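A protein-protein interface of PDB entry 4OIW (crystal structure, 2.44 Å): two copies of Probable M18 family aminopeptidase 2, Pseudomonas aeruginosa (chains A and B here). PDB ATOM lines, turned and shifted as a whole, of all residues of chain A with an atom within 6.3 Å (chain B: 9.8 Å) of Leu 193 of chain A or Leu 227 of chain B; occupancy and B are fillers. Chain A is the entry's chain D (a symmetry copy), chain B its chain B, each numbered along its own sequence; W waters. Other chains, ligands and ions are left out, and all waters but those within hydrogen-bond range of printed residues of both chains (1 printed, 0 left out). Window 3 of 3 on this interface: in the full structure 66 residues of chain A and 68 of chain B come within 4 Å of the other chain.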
ATOM      1  N   LEU A 104      15.903   1.517  15.018  1.00  0.00           N
ATOM      2  CA  LEU A 104      17.124   0.985  14.512  1.00  0.00           C
ATOM      3  C   LEU A 104      17.300   1.577  13.113  1.00  0.00           C
ATOM      4  O   LEU A 104      16.398   1.506  12.297  1.00  0.00           O
ATOM      5  CB  LEU A 104      17.037  -0.530  14.399  1.00  0.00           C
ATOM      6  CG  LEU A 104      18.289  -1.184  13.815  1.00  0.00           C
ATOM      7  CD1 LEU A 104      19.490  -0.857  14.683  1.00  0.00           C
ATOM      8  CD2 LEU A 104      18.081  -2.669  13.745  1.00  0.00           C
ATOM      9  N   LEU A 126      17.444  -4.053   0.479  1.00  0.00           N
ATOM     10  CA  LEU A 126      18.861  -4.165   0.641  1.00  0.00           C
ATOM     11  C   LEU A 126      19.379  -5.365  -0.123  1.00  0.00           C
ATOM     12  O   LEU A 126      18.777  -6.429  -0.067  1.00  0.00           O
ATOM     13  CB  LEU A 126      19.104  -4.341   2.109  1.00  0.00           C
ATOM     14  CG  LEU A 126      20.447  -4.119   2.720  1.00  0.00           C
ATOM     15  CD1 LEU A 126      21.056  -2.862   2.126  1.00  0.00           C
ATOM     16  CD2 LEU A 126      20.232  -3.946   4.225  1.00  0.00           C
ATOM     17  N   PHE A 145      17.164  -8.901   0.062  1.00  0.00           N
ATOM     18  CA  PHE A 145      16.020  -9.060   1.000  1.00  0.00           C
ATOM     19  C   PHE A 145      14.661  -8.944   0.369  1.00  0.00           C
ATOM     20  O   PHE A 145      13.669  -9.403   0.944  1.00  0.00           O
ATOM     21  CB  PHE A 145      16.087  -8.023   2.093  1.00  0.00           C
ATOM     22  CG  PHE A 145      17.116  -8.319   3.106  1.00  0.00           C
ATOM     23  CD1 PHE A 145      18.450  -8.046   2.850  1.00  0.00           C
ATOM     24  CD2 PHE A 145      16.763  -8.882   4.315  1.00  0.00           C
ATOM     25  CE1 PHE A 145      19.425  -8.327   3.792  1.00  0.00           C
ATOM     26  CE2 PHE A 145      17.733  -9.169   5.258  1.00  0.00           C
ATOM     27  CZ  PHE A 145      19.065  -8.891   5.000  1.00  0.00           C
ATOM     28  N   LYS A 147      11.935  -7.616   0.248  1.00  0.00           N
ATOM     29  CA  LYS A 147      10.964  -6.856   1.043  1.00  0.00           C
ATOM     30  C   LYS A 147      11.401  -5.378   1.293  1.00  0.00           C
ATOM     31  O   LYS A 147      12.595  -5.058   1.448  1.00  0.00           O
ATOM     32  CB  LYS A 147      10.817  -7.575   2.365  1.00  0.00           C
ATOM     33  CG  LYS A 147       9.590  -7.239   3.156  1.00  0.00           C
ATOM     34  CD  LYS A 147       9.777  -7.706   4.624  1.00  0.00           C
ATOM     35  CE  LYS A 147       8.789  -7.044   5.604  1.00  0.00           C
ATOM     36  NZ  LYS A 147       7.441  -6.772   5.001  1.00  0.00           N
ATOM     37  N   ALA A 148      10.412  -4.491   1.324  1.00  0.00           N
ATOM     38  CA  ALA A 148      10.630  -3.090   1.657  1.00  0.00           C
ATOM     39  C   ALA A 148      10.797  -2.984   3.144  1.00  0.00           C
ATOM     40  O   ALA A 148       9.808  -2.938   3.884  1.00  0.00           O
ATOM     41  CB  ALA A 148       9.464  -2.233   1.204  1.00  0.00           C
ATOM     42  N   ILE A 149      12.049  -2.907   3.571  1.00  0.00           N
ATOM     43  CA  ILE A 149      12.393  -2.932   4.995  1.00  0.00           C
ATOM     44  C   ILE A 149      13.033  -1.652   5.522  1.00  0.00           C
ATOM     45  O   ILE A 149      13.352  -1.584   6.716  1.00  0.00           O
ATOM     46  CB  ILE A 149      13.419  -4.052   5.286  1.00  0.00           C
ATOM     47  CG1 ILE A 149      14.632  -3.920   4.372  1.00  0.00           C
ATOM     48  CG2 ILE A 149      12.781  -5.413   5.079  1.00  0.00           C
ATOM     49  CD1 ILE A 149      15.849  -4.648   4.891  1.00  0.00           C
ATOM     50  N   ALA A 150      13.267  -0.664   4.646  1.00  0.00           N
ATOM     51  CA  ALA A 150      13.912   0.597   5.052  1.00  0.00           C
ATOM     52  C   ALA A 150      13.259   1.788   4.417  1.00  0.00           C
ATOM     53  O   ALA A 150      12.694   1.702   3.337  1.00  0.00           O
ATOM     54  CB  ALA A 150      15.380   0.597   4.690  1.00  0.00           C
ATOM     55  N   ILE A 179      15.013   0.987   9.746  1.00  0.00           N
ATOM     56  CA  ILE A 179      14.632  -0.398   9.350  1.00  0.00           C
ATOM     57  C   ILE A 179      13.679  -1.107  10.312  1.00  0.00           C
ATOM     58  O   ILE A 179      12.890  -1.949   9.894  1.00  0.00           O
ATOM     59  CB  ILE A 179      15.858  -1.302   9.049  1.00  0.00           C
ATOM     60  CG1 ILE A 179      16.682  -1.563  10.290  1.00  0.00           C
ATOM     61  CG2 ILE A 179      16.777  -0.651   7.998  1.00  0.00           C
ATOM     62  CD1 ILE A 179      17.860  -2.468  10.022  1.00  0.00           C
ATOM     63  N   ALA A 180      13.673  -0.691  11.567  1.00  0.00           N
ATOM     64  CA  ALA A 180      12.829  -1.312  12.571  1.00  0.00           C
ATOM     65  C   ALA A 180      12.665  -0.396  13.769  1.00  0.00           C
ATOM     66  O   ALA A 180      13.305   0.652  13.825  1.00  0.00           O
ATOM     67  CB  ALA A 180      13.457  -2.653  13.017  1.00  0.00           C
ATOM     68  N   ASP A 189      21.911  -6.505  16.009  1.00  0.00           N
ATOM     69  CA  ASP A 189      23.131  -6.882  15.365  1.00  0.00           C
ATOM     70  C   ASP A 189      22.831  -7.172  13.902  1.00  0.00           C
ATOM     71  O   ASP A 189      22.222  -8.179  13.564  1.00  0.00           O
ATOM     72  CB  ASP A 189      23.754  -8.089  16.053  1.00  0.00           C
ATOM     73  CG  ASP A 189      25.130  -8.480  15.448  1.00  0.00           C
ATOM     74  OD1 ASP A 189      25.415  -8.086  14.298  1.00  0.00           O
ATOM     75  OD2 ASP A 189      25.918  -9.183  16.127  1.00  0.00           O
ATOM     76  N   PHE A 190      23.291  -6.275  13.045  1.00  0.00           N
ATOM     77  CA  PHE A 190      23.087  -6.379  11.613  1.00  0.00           C
ATOM     78  C   PHE A 190      23.650  -7.686  11.063  1.00  0.00           C
ATOM     79  O   PHE A 190      23.070  -8.301  10.159  1.00  0.00           O
ATOM     80  CB  PHE A 190      23.736  -5.180  10.874  1.00  0.00           C
ATOM     81  CG  PHE A 190      23.466  -5.174   9.373  1.00  0.00           C
ATOM     82  CD1 PHE A 190      22.170  -5.175   8.888  1.00  0.00           C
ATOM     83  CD2 PHE A 190      24.492  -5.257   8.485  1.00  0.00           C
ATOM     84  CE1 PHE A 190      21.895  -5.198   7.538  1.00  0.00           C
ATOM     85  CE2 PHE A 190      24.246  -5.259   7.133  1.00  0.00           C
ATOM     86  CZ  PHE A 190      22.949  -5.240   6.643  1.00  0.00           C
ATOM     87  N   ARG A 191      24.793  -8.110  11.581  1.00  0.00           N
ATOM     88  CA  ARG A 191      25.419  -9.320  11.071  1.00  0.00           C
ATOM     89  C   ARG A 191      24.541 -10.567  11.308  1.00  0.00           C
ATOM     90  O   ARG A 191      24.476 -11.438  10.461  1.00  0.00           O
ATOM     91  CB  ARG A 191      26.820  -9.461  11.626  1.00  0.00           C
ATOM     92  CG  ARG A 191      27.798  -8.560  10.891  1.00  0.00           C
ATOM     93  CD  ARG A 191      29.131  -8.401  11.615  1.00  0.00           C
ATOM     94  NE  ARG A 191      30.134  -7.778  10.740  1.00  0.00           N
ATOM     95  CZ  ARG A 191      30.201  -6.477  10.437  1.00  0.00           C
ATOM     96  NH1 ARG A 191      29.291  -5.622  10.904  1.00  0.00           N
ATOM     97  NH2 ARG A 191      31.168  -6.031   9.629  1.00  0.00           N
ATOM     98  N   LEU A 192      23.834 -10.620  12.434  1.00  0.00           N
ATOM     99  CA  LEU A 192      22.899 -11.728  12.728  1.00  0.00           C
ATOM    100  C   LEU A 192      21.784 -11.758  11.688  1.00  0.00           C
ATOM    101  O   LEU A 192      21.321 -12.823  11.267  1.00  0.00           O
ATOM    102  CB  LEU A 192      22.308 -11.594  14.122  1.00  0.00           C
ATOM    103  CG  LEU A 192      22.849 -12.513  15.230  1.00  0.00           C
ATOM    104  CD1 LEU A 192      24.321 -12.863  15.099  1.00  0.00           C
ATOM    105  CD2 LEU A 192      22.555 -11.933  16.615  1.00  0.00           C
ATOM    106  N   LEU A 193      21.400 -10.580  11.224  1.00  0.00           N
ATOM    107  CA  LEU A 193      20.357 -10.494  10.222  1.00  0.00           C
ATOM    108  C   LEU A 193      20.821 -11.052   8.869  1.00  0.00           C
ATOM    109  O   LEU A 193      20.062 -11.722   8.157  1.00  0.00           O
ATOM    110  CB  LEU A 193      19.962  -9.054  10.067  1.00  0.00           C
ATOM    111  CG  LEU A 193      18.561  -8.895   9.597  1.00  0.00           C
ATOM    112  CD1 LEU A 193      17.684  -8.930  10.850  1.00  0.00           C
ATOM    113  CD2 LEU A 193      18.494  -7.589   8.845  1.00  0.00           C
ATOM    114  N   LEU A 194      22.081 -10.798   8.529  1.00  0.00           N
ATOM    115  CA  LEU A 194      22.641 -11.349   7.313  1.00  0.00           C
ATOM    116  C   LEU A 194      22.842 -12.868   7.431  1.00  0.00           C
ATOM    117  O   LEU A 194      22.724 -13.579   6.440  1.00  0.00           O
ATOM    118  CB  LEU A 194      23.955 -10.683   6.997  1.00  0.00           C
ATOM    119  CG  LEU A 194      23.942  -9.198   6.676  1.00  0.00           C
ATOM    120  CD1 LEU A 194      25.374  -8.644   6.583  1.00  0.00           C
ATOM    121  CD2 LEU A 194      23.145  -8.945   5.410  1.00  0.00           C
ATOM    122  N   ASP A 195      23.158 -13.347   8.635  1.00  0.00           N
ATOM    123  CA  ASP A 195      23.294 -14.785   8.895  1.00  0.00           C
ATOM    124  C   ASP A 195      21.957 -15.476   8.530  1.00  0.00           C
ATOM    125  O   ASP A 195      21.945 -16.406   7.757  1.00  0.00           O
ATOM    126  CB  ASP A 195      23.757 -14.985  10.360  1.00  0.00           C
ATOM    127  CG  ASP A 195      23.723 -16.413  10.816  1.00  0.00           C
ATOM    128  OD1 ASP A 195      22.626 -16.955  11.056  1.00  0.00           O
ATOM    129  OD2 ASP A 195      24.799 -16.995  10.982  1.00  0.00           O
ATOM    130  N   GLU A 196      20.841 -14.961   9.017  1.00  0.00           N
ATOM    131  CA  GLU A 196      19.509 -15.465   8.647  1.00  0.00           C
ATOM    132  C   GLU A 196      19.263 -15.409   7.154  1.00  0.00           C
ATOM    133  O   GLU A 196      18.773 -16.367   6.555  1.00  0.00           O
ATOM    134  CB  GLU A 196      18.391 -14.656   9.314  1.00  0.00           C
ATOM    135  CG  GLU A 196      18.478 -14.589  10.816  1.00  0.00           C
ATOM    136  CD  GLU A 196      17.348 -13.766  11.454  1.00  0.00           C
ATOM    137  OE1 GLU A 196      16.323 -13.464  10.777  1.00  0.00           O
ATOM    138  OE2 GLU A 196      17.501 -13.424  12.650  1.00  0.00           O
ATOM    139  N   GLN A 197      19.601 -14.295   6.532  1.00  0.00           N
ATOM    140  CA  GLN A 197      19.326 -14.188   5.098  1.00  0.00           C
ATOM    141  C   GLN A 197      20.143 -15.187   4.320  1.00  0.00           C
ATOM    142  O   GLN A 197      19.661 -15.696   3.345  1.00  0.00           O
ATOM    143  CB  GLN A 197      19.584 -12.794   4.577  1.00  0.00           C
ATOM    144  CG  GLN A 197      19.069 -12.534   3.161  1.00  0.00           C
ATOM    145  CD  GLN A 197      17.552 -12.658   3.041  1.00  0.00           C
ATOM    146  OE1 GLN A 197      16.839 -12.583   4.010  1.00  0.00           O
ATOM    147  NE2 GLN A 197      17.074 -12.842   1.838  1.00  0.00           N
ATOM    148  N   LEU A 198      21.371 -15.461   4.743  1.00  0.00           N
ATOM    149  CA  LEU A 198      22.184 -16.536   4.141  1.00  0.00           C
ATOM    150  C   LEU A 198      21.533 -17.918   4.249  1.00  0.00           C
ATOM    151  O   LEU A 198      21.531 -18.687   3.286  1.00  0.00           O
ATOM    152  CB  LEU A 198      23.562 -16.616   4.782  1.00  0.00           C
ATOM    153  CG  LEU A 198      24.497 -15.474   4.353  1.00  0.00           C
ATOM    154  CD1 LEU A 198      25.699 -15.521   5.274  1.00  0.00           C
ATOM    155  CD2 LEU A 198      24.936 -15.579   2.896  1.00  0.00           C
ATOM    156  N   ARG A 200      18.161 -18.533   4.699  1.00  0.00           N
ATOM    157  CA  ARG A 200      16.999 -18.580   3.828  1.00  0.00           C
ATOM    158  C   ARG A 200      17.310 -18.614   2.328  1.00  0.00           C
ATOM    159  O   ARG A 200      16.608 -19.256   1.552  1.00  0.00           O
ATOM    160  CB  ARG A 200      16.149 -17.355   3.989  1.00  0.00           C
ATOM    161  CG  ARG A 200      15.470 -17.197   5.296  1.00  0.00           C
ATOM    162  CD  ARG A 200      14.486 -16.026   5.172  1.00  0.00           C
ATOM    163  NE  ARG A 200      14.338 -15.512   6.503  1.00  0.00           N
ATOM    164  CZ  ARG A 200      15.008 -14.496   7.038  1.00  0.00           C
ATOM    165  NH1 ARG A 200      15.840 -13.749   6.346  1.00  0.00           N
ATOM    166  NH2 ARG A 200      14.786 -14.206   8.308  1.00  0.00           N
ATOM    167  N   MET B   3       5.486 -11.069   9.506  1.00  0.00           N
ATOM    168  CA  MET B   3       4.904 -10.239   8.393  1.00  0.00           C
ATOM    169  C   MET B   3       3.383  -9.918   8.625  1.00  0.00           C
ATOM    170  O   MET B   3       3.025  -8.900   9.309  1.00  0.00           O
ATOM    171  CB  MET B   3       5.178 -10.946   7.042  1.00  0.00           C
ATOM    172  CG  MET B   3       5.956 -10.117   6.034  1.00  0.00           C
ATOM    173  SD  MET B   3       6.948 -11.164   4.944  1.00  0.00           S
ATOM    174  CE  MET B   3       8.169 -11.868   6.057  1.00  0.00           C
ATOM    175  N   ARG B   4       2.528 -10.765   8.044  1.00  0.00           N
ATOM    176  CA  ARG B   4       1.143 -10.895   8.440  1.00  0.00           C
ATOM    177  C   ARG B   4       0.323  -9.867   7.718  1.00  0.00           C
ATOM    178  O   ARG B   4       0.281  -9.946   6.485  1.00  0.00           O
ATOM    179  CB  ARG B   4       0.946 -10.926   9.964  1.00  0.00           C
ATOM    180  CG  ARG B   4      -0.458 -11.359  10.344  1.00  0.00           C
ATOM    181  CD  ARG B   4      -1.101 -10.893  11.651  1.00  0.00           C
ATOM    182  NE  ARG B   4      -2.516 -11.150  11.396  1.00  0.00           N
ATOM    183  CZ  ARG B   4      -3.540 -10.574  11.986  1.00  0.00           C
ATOM    184  NH1 ARG B   4      -3.359  -9.691  12.956  1.00  0.00           N
ATOM    185  NH2 ARG B   4      -4.755 -10.905  11.591  1.00  0.00           N
ATOM    186  N   VAL B 224       2.865  -1.474   3.714  1.00  0.00           N
ATOM    187  CA  VAL B 224       3.515  -1.715   4.982  1.00  0.00           C
ATOM    188  C   VAL B 224       5.017  -1.858   4.714  1.00  0.00           C
ATOM    189  O   VAL B 224       5.419  -2.535   3.774  1.00  0.00           O
ATOM    190  CB  VAL B 224       2.955  -2.989   5.605  1.00  0.00           C
ATOM    191  CG1 VAL B 224       3.489  -3.178   7.015  1.00  0.00           C
ATOM    192  CG2 VAL B 224       1.454  -2.874   5.642  1.00  0.00           C
ATOM    193  N   VAL B 225       5.843  -1.189   5.508  1.00  0.00           N
ATOM    194  CA  VAL B 225       7.260  -1.246   5.261  1.00  0.00           C
ATOM    195  C   VAL B 225       7.995  -1.422   6.590  1.00  0.00           C
ATOM    196  O   VAL B 225       7.419  -1.276   7.681  1.00  0.00           O
ATOM    197  CB  VAL B 225       7.779  -0.013   4.438  1.00  0.00           C
ATOM    198  CG1 VAL B 225       6.908   0.264   3.225  1.00  0.00           C
ATOM    199  CG2 VAL B 225       7.853   1.229   5.292  1.00  0.00           C
ATOM    200  N   GLY B 226       9.255  -1.785   6.478  1.00  0.00           N
ATOM    201  CA  GLY B 226      10.086  -2.066   7.611  1.00  0.00           C
ATOM    202  C   GLY B 226      10.372  -3.552   7.792  1.00  0.00           C
ATOM    203  O   GLY B 226       9.574  -4.394   7.402  1.00  0.00           O
ATOM    204  N   LEU B 227      11.500  -3.855   8.433  1.00  0.00           N
ATOM    205  CA  LEU B 227      11.886  -5.224   8.791  1.00  0.00           C
ATOM    206  C   LEU B 227      10.822  -6.014   9.579  1.00  0.00           C
ATOM    207  O   LEU B 227      10.631  -7.169   9.282  1.00  0.00           O
ATOM    208  CB  LEU B 227      13.145  -5.170   9.597  1.00  0.00           C
ATOM    209  CG  LEU B 227      13.900  -6.466   9.777  1.00  0.00           C
ATOM    210  CD1 LEU B 227      14.525  -6.896   8.462  1.00  0.00           C
ATOM    211  CD2 LEU B 227      14.964  -6.231  10.854  1.00  0.00           C
ATOM    212  N   ASN B 228      10.128  -5.414  10.543  1.00  0.00           N
ATOM    213  CA  ASN B 228       9.030  -6.111  11.239  1.00  0.00           C
ATOM    214  C   ASN B 228       7.661  -5.528  10.920  1.00  0.00           C
ATOM    215  O   ASN B 228       6.726  -5.598  11.727  1.00  0.00           O
ATOM    216  CB  ASN B 228       9.256  -6.171  12.767  1.00  0.00           C
ATOM    217  CG  ASN B 228      10.683  -6.518  13.119  1.00  0.00           C
ATOM    218  OD1 ASN B 228      11.127  -7.640  12.951  1.00  0.00           O
ATOM    219  ND2 ASN B 228      11.435  -5.528  13.537  1.00  0.00           N
ATOM    220  N   ASP B 229       7.514  -4.969   9.729  1.00  0.00           N
ATOM    221  CA  ASP B 229       6.255  -4.302   9.357  1.00  0.00           C
ATOM    222  C   ASP B 229       5.792  -3.224  10.332  1.00  0.00           C
ATOM    223  O   ASP B 229       4.615  -3.062  10.581  1.00  0.00           O
ATOM    224  CB  ASP B 229       5.180  -5.353   9.170  1.00  0.00           C
ATOM    225  CG  ASP B 229       5.433  -6.225   7.895  1.00  0.00           C
ATOM    226  OD1 ASP B 229       6.246  -5.871   7.067  1.00  0.00           O
ATOM    227  OD2 ASP B 229       4.823  -7.272   7.703  1.00  0.00           O
ATOM    228  N   GLU B 230       6.728  -2.424  10.827  1.00  0.00           N
ATOM    229  CA  GLU B 230       6.389  -1.370  11.779  1.00  0.00           C
ATOM    230  C   GLU B 230       5.660  -0.163  11.200  1.00  0.00           C
ATOM    231  O   GLU B 230       5.058   0.599  11.987  1.00  0.00           O
ATOM    232  CB  GLU B 230       7.663  -0.865  12.478  1.00  0.00           C
ATOM    233  CG  GLU B 230       8.320  -1.912  13.351  1.00  0.00           C
ATOM    234  CD  GLU B 230       9.494  -2.637  12.703  1.00  0.00           C
ATOM    235  OE1 GLU B 230       9.519  -2.887  11.435  1.00  0.00           O
ATOM    236  OE2 GLU B 230      10.387  -2.994  13.504  1.00  0.00           O
ATOM    237  N   PHE B 231       5.728   0.050   9.877  1.00  0.00           N
ATOM    238  CA  PHE B 231       5.287   1.312   9.302  1.00  0.00           C
ATOM    239  C   PHE B 231       4.392   1.167   8.103  1.00  0.00           C
ATOM    240  O   PHE B 231       4.371   0.144   7.446  1.00  0.00           O
ATOM    241  CB  PHE B 231       6.467   2.214   8.915  1.00  0.00           C
ATOM    242  CG  PHE B 231       7.625   2.151   9.879  1.00  0.00           C
ATOM    243  CD1 PHE B 231       7.541   2.732  11.130  1.00  0.00           C
ATOM    244  CD2 PHE B 231       8.800   1.526   9.523  1.00  0.00           C
ATOM    245  CE1 PHE B 231       8.596   2.651  12.029  1.00  0.00           C
ATOM    246  CE2 PHE B 231       9.857   1.438  10.420  1.00  0.00           C
ATOM    247  CZ  PHE B 231       9.757   1.995  11.675  1.00  0.00           C
ATOM    248  N   SER B 411       2.273   1.144  11.847  1.00  0.00           N
ATOM    249  CA  SER B 411       1.301   0.119  11.481  1.00  0.00           C
ATOM    250  C   SER B 411       0.396  -0.382  12.646  1.00  0.00           C
ATOM    251  O   SER B 411      -0.596  -1.021  12.383  1.00  0.00           O
ATOM    252  CB  SER B 411       2.031  -1.053  10.848  1.00  0.00           C
ATOM    253  OG  SER B 411       2.799  -1.681  11.874  1.00  0.00           O
HETATM  254  O   HOH W   1       7.429  -4.513   3.363  1.00  0.00           O
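The backbone NH (N) of Gly 226 of chain B is in hydrogen-bond range of the backbone carbonyl oxygen (O) of Ala 148 of chain A, 2.9 Å away. The backbone carbonyl oxygen (O) of Ile 179 of chain A is in hydrogen-bond range of the backbone NH (N) of Leu 227 of chain B, 2.8 Å away. OD1 of Asp 229 of chain B is in salt-bridge range of NZ of Lys 147 of chain A (2.6 Å). N of Leu 227 of chain B sits at hydrogen-bond distance from O of Ile 149 of chain A.
Hydrophobic or aromatic side chains of chain A within 4 Å of the printed part of chain B: Ile 149, Ala 180 and Leu 193. Printed residues of chain B that touch a printed residue of chain A: Met 3, Val 225, Gly 226, Leu 227, Asn 228, Asp 229 and Glu 230. Hydrophobic or aromatic side chains of chain B that line the printed part of chain A: Met 3, Val 225 and Leu 227. Along chain B the printed residues that touch a printed residue of chain A span positions 3 to 230.
Water W1 lies within hydrogen-bond range of NZ of Lys 147 of chain A, O of Val 224 of chain B and O of Ala 148 of chain A.
Among the printed residues, pairs that only touch across the chains: Ala 180 of chain A with Glu 230 of chain B, Lys 147 of chain A with Gly 226 of chain B, Ala 148 of chain A with Val 225 of chain B, Ile 149 of chain A with Gly 226 of chain B, Ala 180 of chain A with Asn 228 of chain B, Ile 179 of chain A with Gly 226 of chain B, Lys 147 of chain A with Met 3 of chain B, Ile 179 of chain A with Glu 230 of chain B and Leu 193 of chain A with Leu 227 of chain B.
N of Val 225 of chain B sits at hydrogen-bond distance from O of Phe 231 of chain B, at 2.8 Å. The backbone carbonyl oxygen (O) of Leu 104 of chain A sits at hydrogen-bond distance from the backbone NH (N) of Ile 179 of chain A. OG of Ser 411 of chain B lies within hydrogen-bond range of O of Asp 229 of chain B (2.6 Å). O of Val 225 of chain B is in hydrogen-bond range of N of Glu 230 of chain B, 3.4 Å away. OE2 of Glu 230 of chain B lies within hydrogen-bond range of ND2 of Asn 228 of chain B (2.7 Å). N of Ser 411 of chain B sits at hydrogen-bond distance from O of Glu 230 of chain B (2.8 Å).
Of the printed residues of chain B, Leu 193 of chain A touches Leu 227 (3.8 Å). Of the printed residues of chain A, Leu 227 of chain B touches Ile 149, Ile 179 and Leu 193. Ile 149 of chain A touches just these residues of chain B: Gly 226 (3.4 Å) and Leu 227 (3.4 Å). No residue of chain B comes within 4 Å of Leu 192 of chain A. No residue of chain B comes within 4 Å of Leu 194 of chain A. Of the printed residues of chain B, Lys 147 of chain A touches Met 3, Gly 226 and Asp 229. Of the printed residues of chain A, Asp 229 of chain B touches Lys 147 (2.6 Å). Asp 189 of chain A touches none of the printed residues of chain B. Leu 198 of chain A touches none of the printed residues of chain B. The nearest residue of chain A that does not touch Leu 227 of chain B is Lys 147 of chain A (4.1 Å). The nearest printed residue of chain A that does not touch Gly 226 of chain B is Ala 150 of chain A (4.6 Å).
No position is printed for both chains. Of the 13 pairs that touch across the chains among the printed residues, none has its exchanged pair printed and touching as well.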
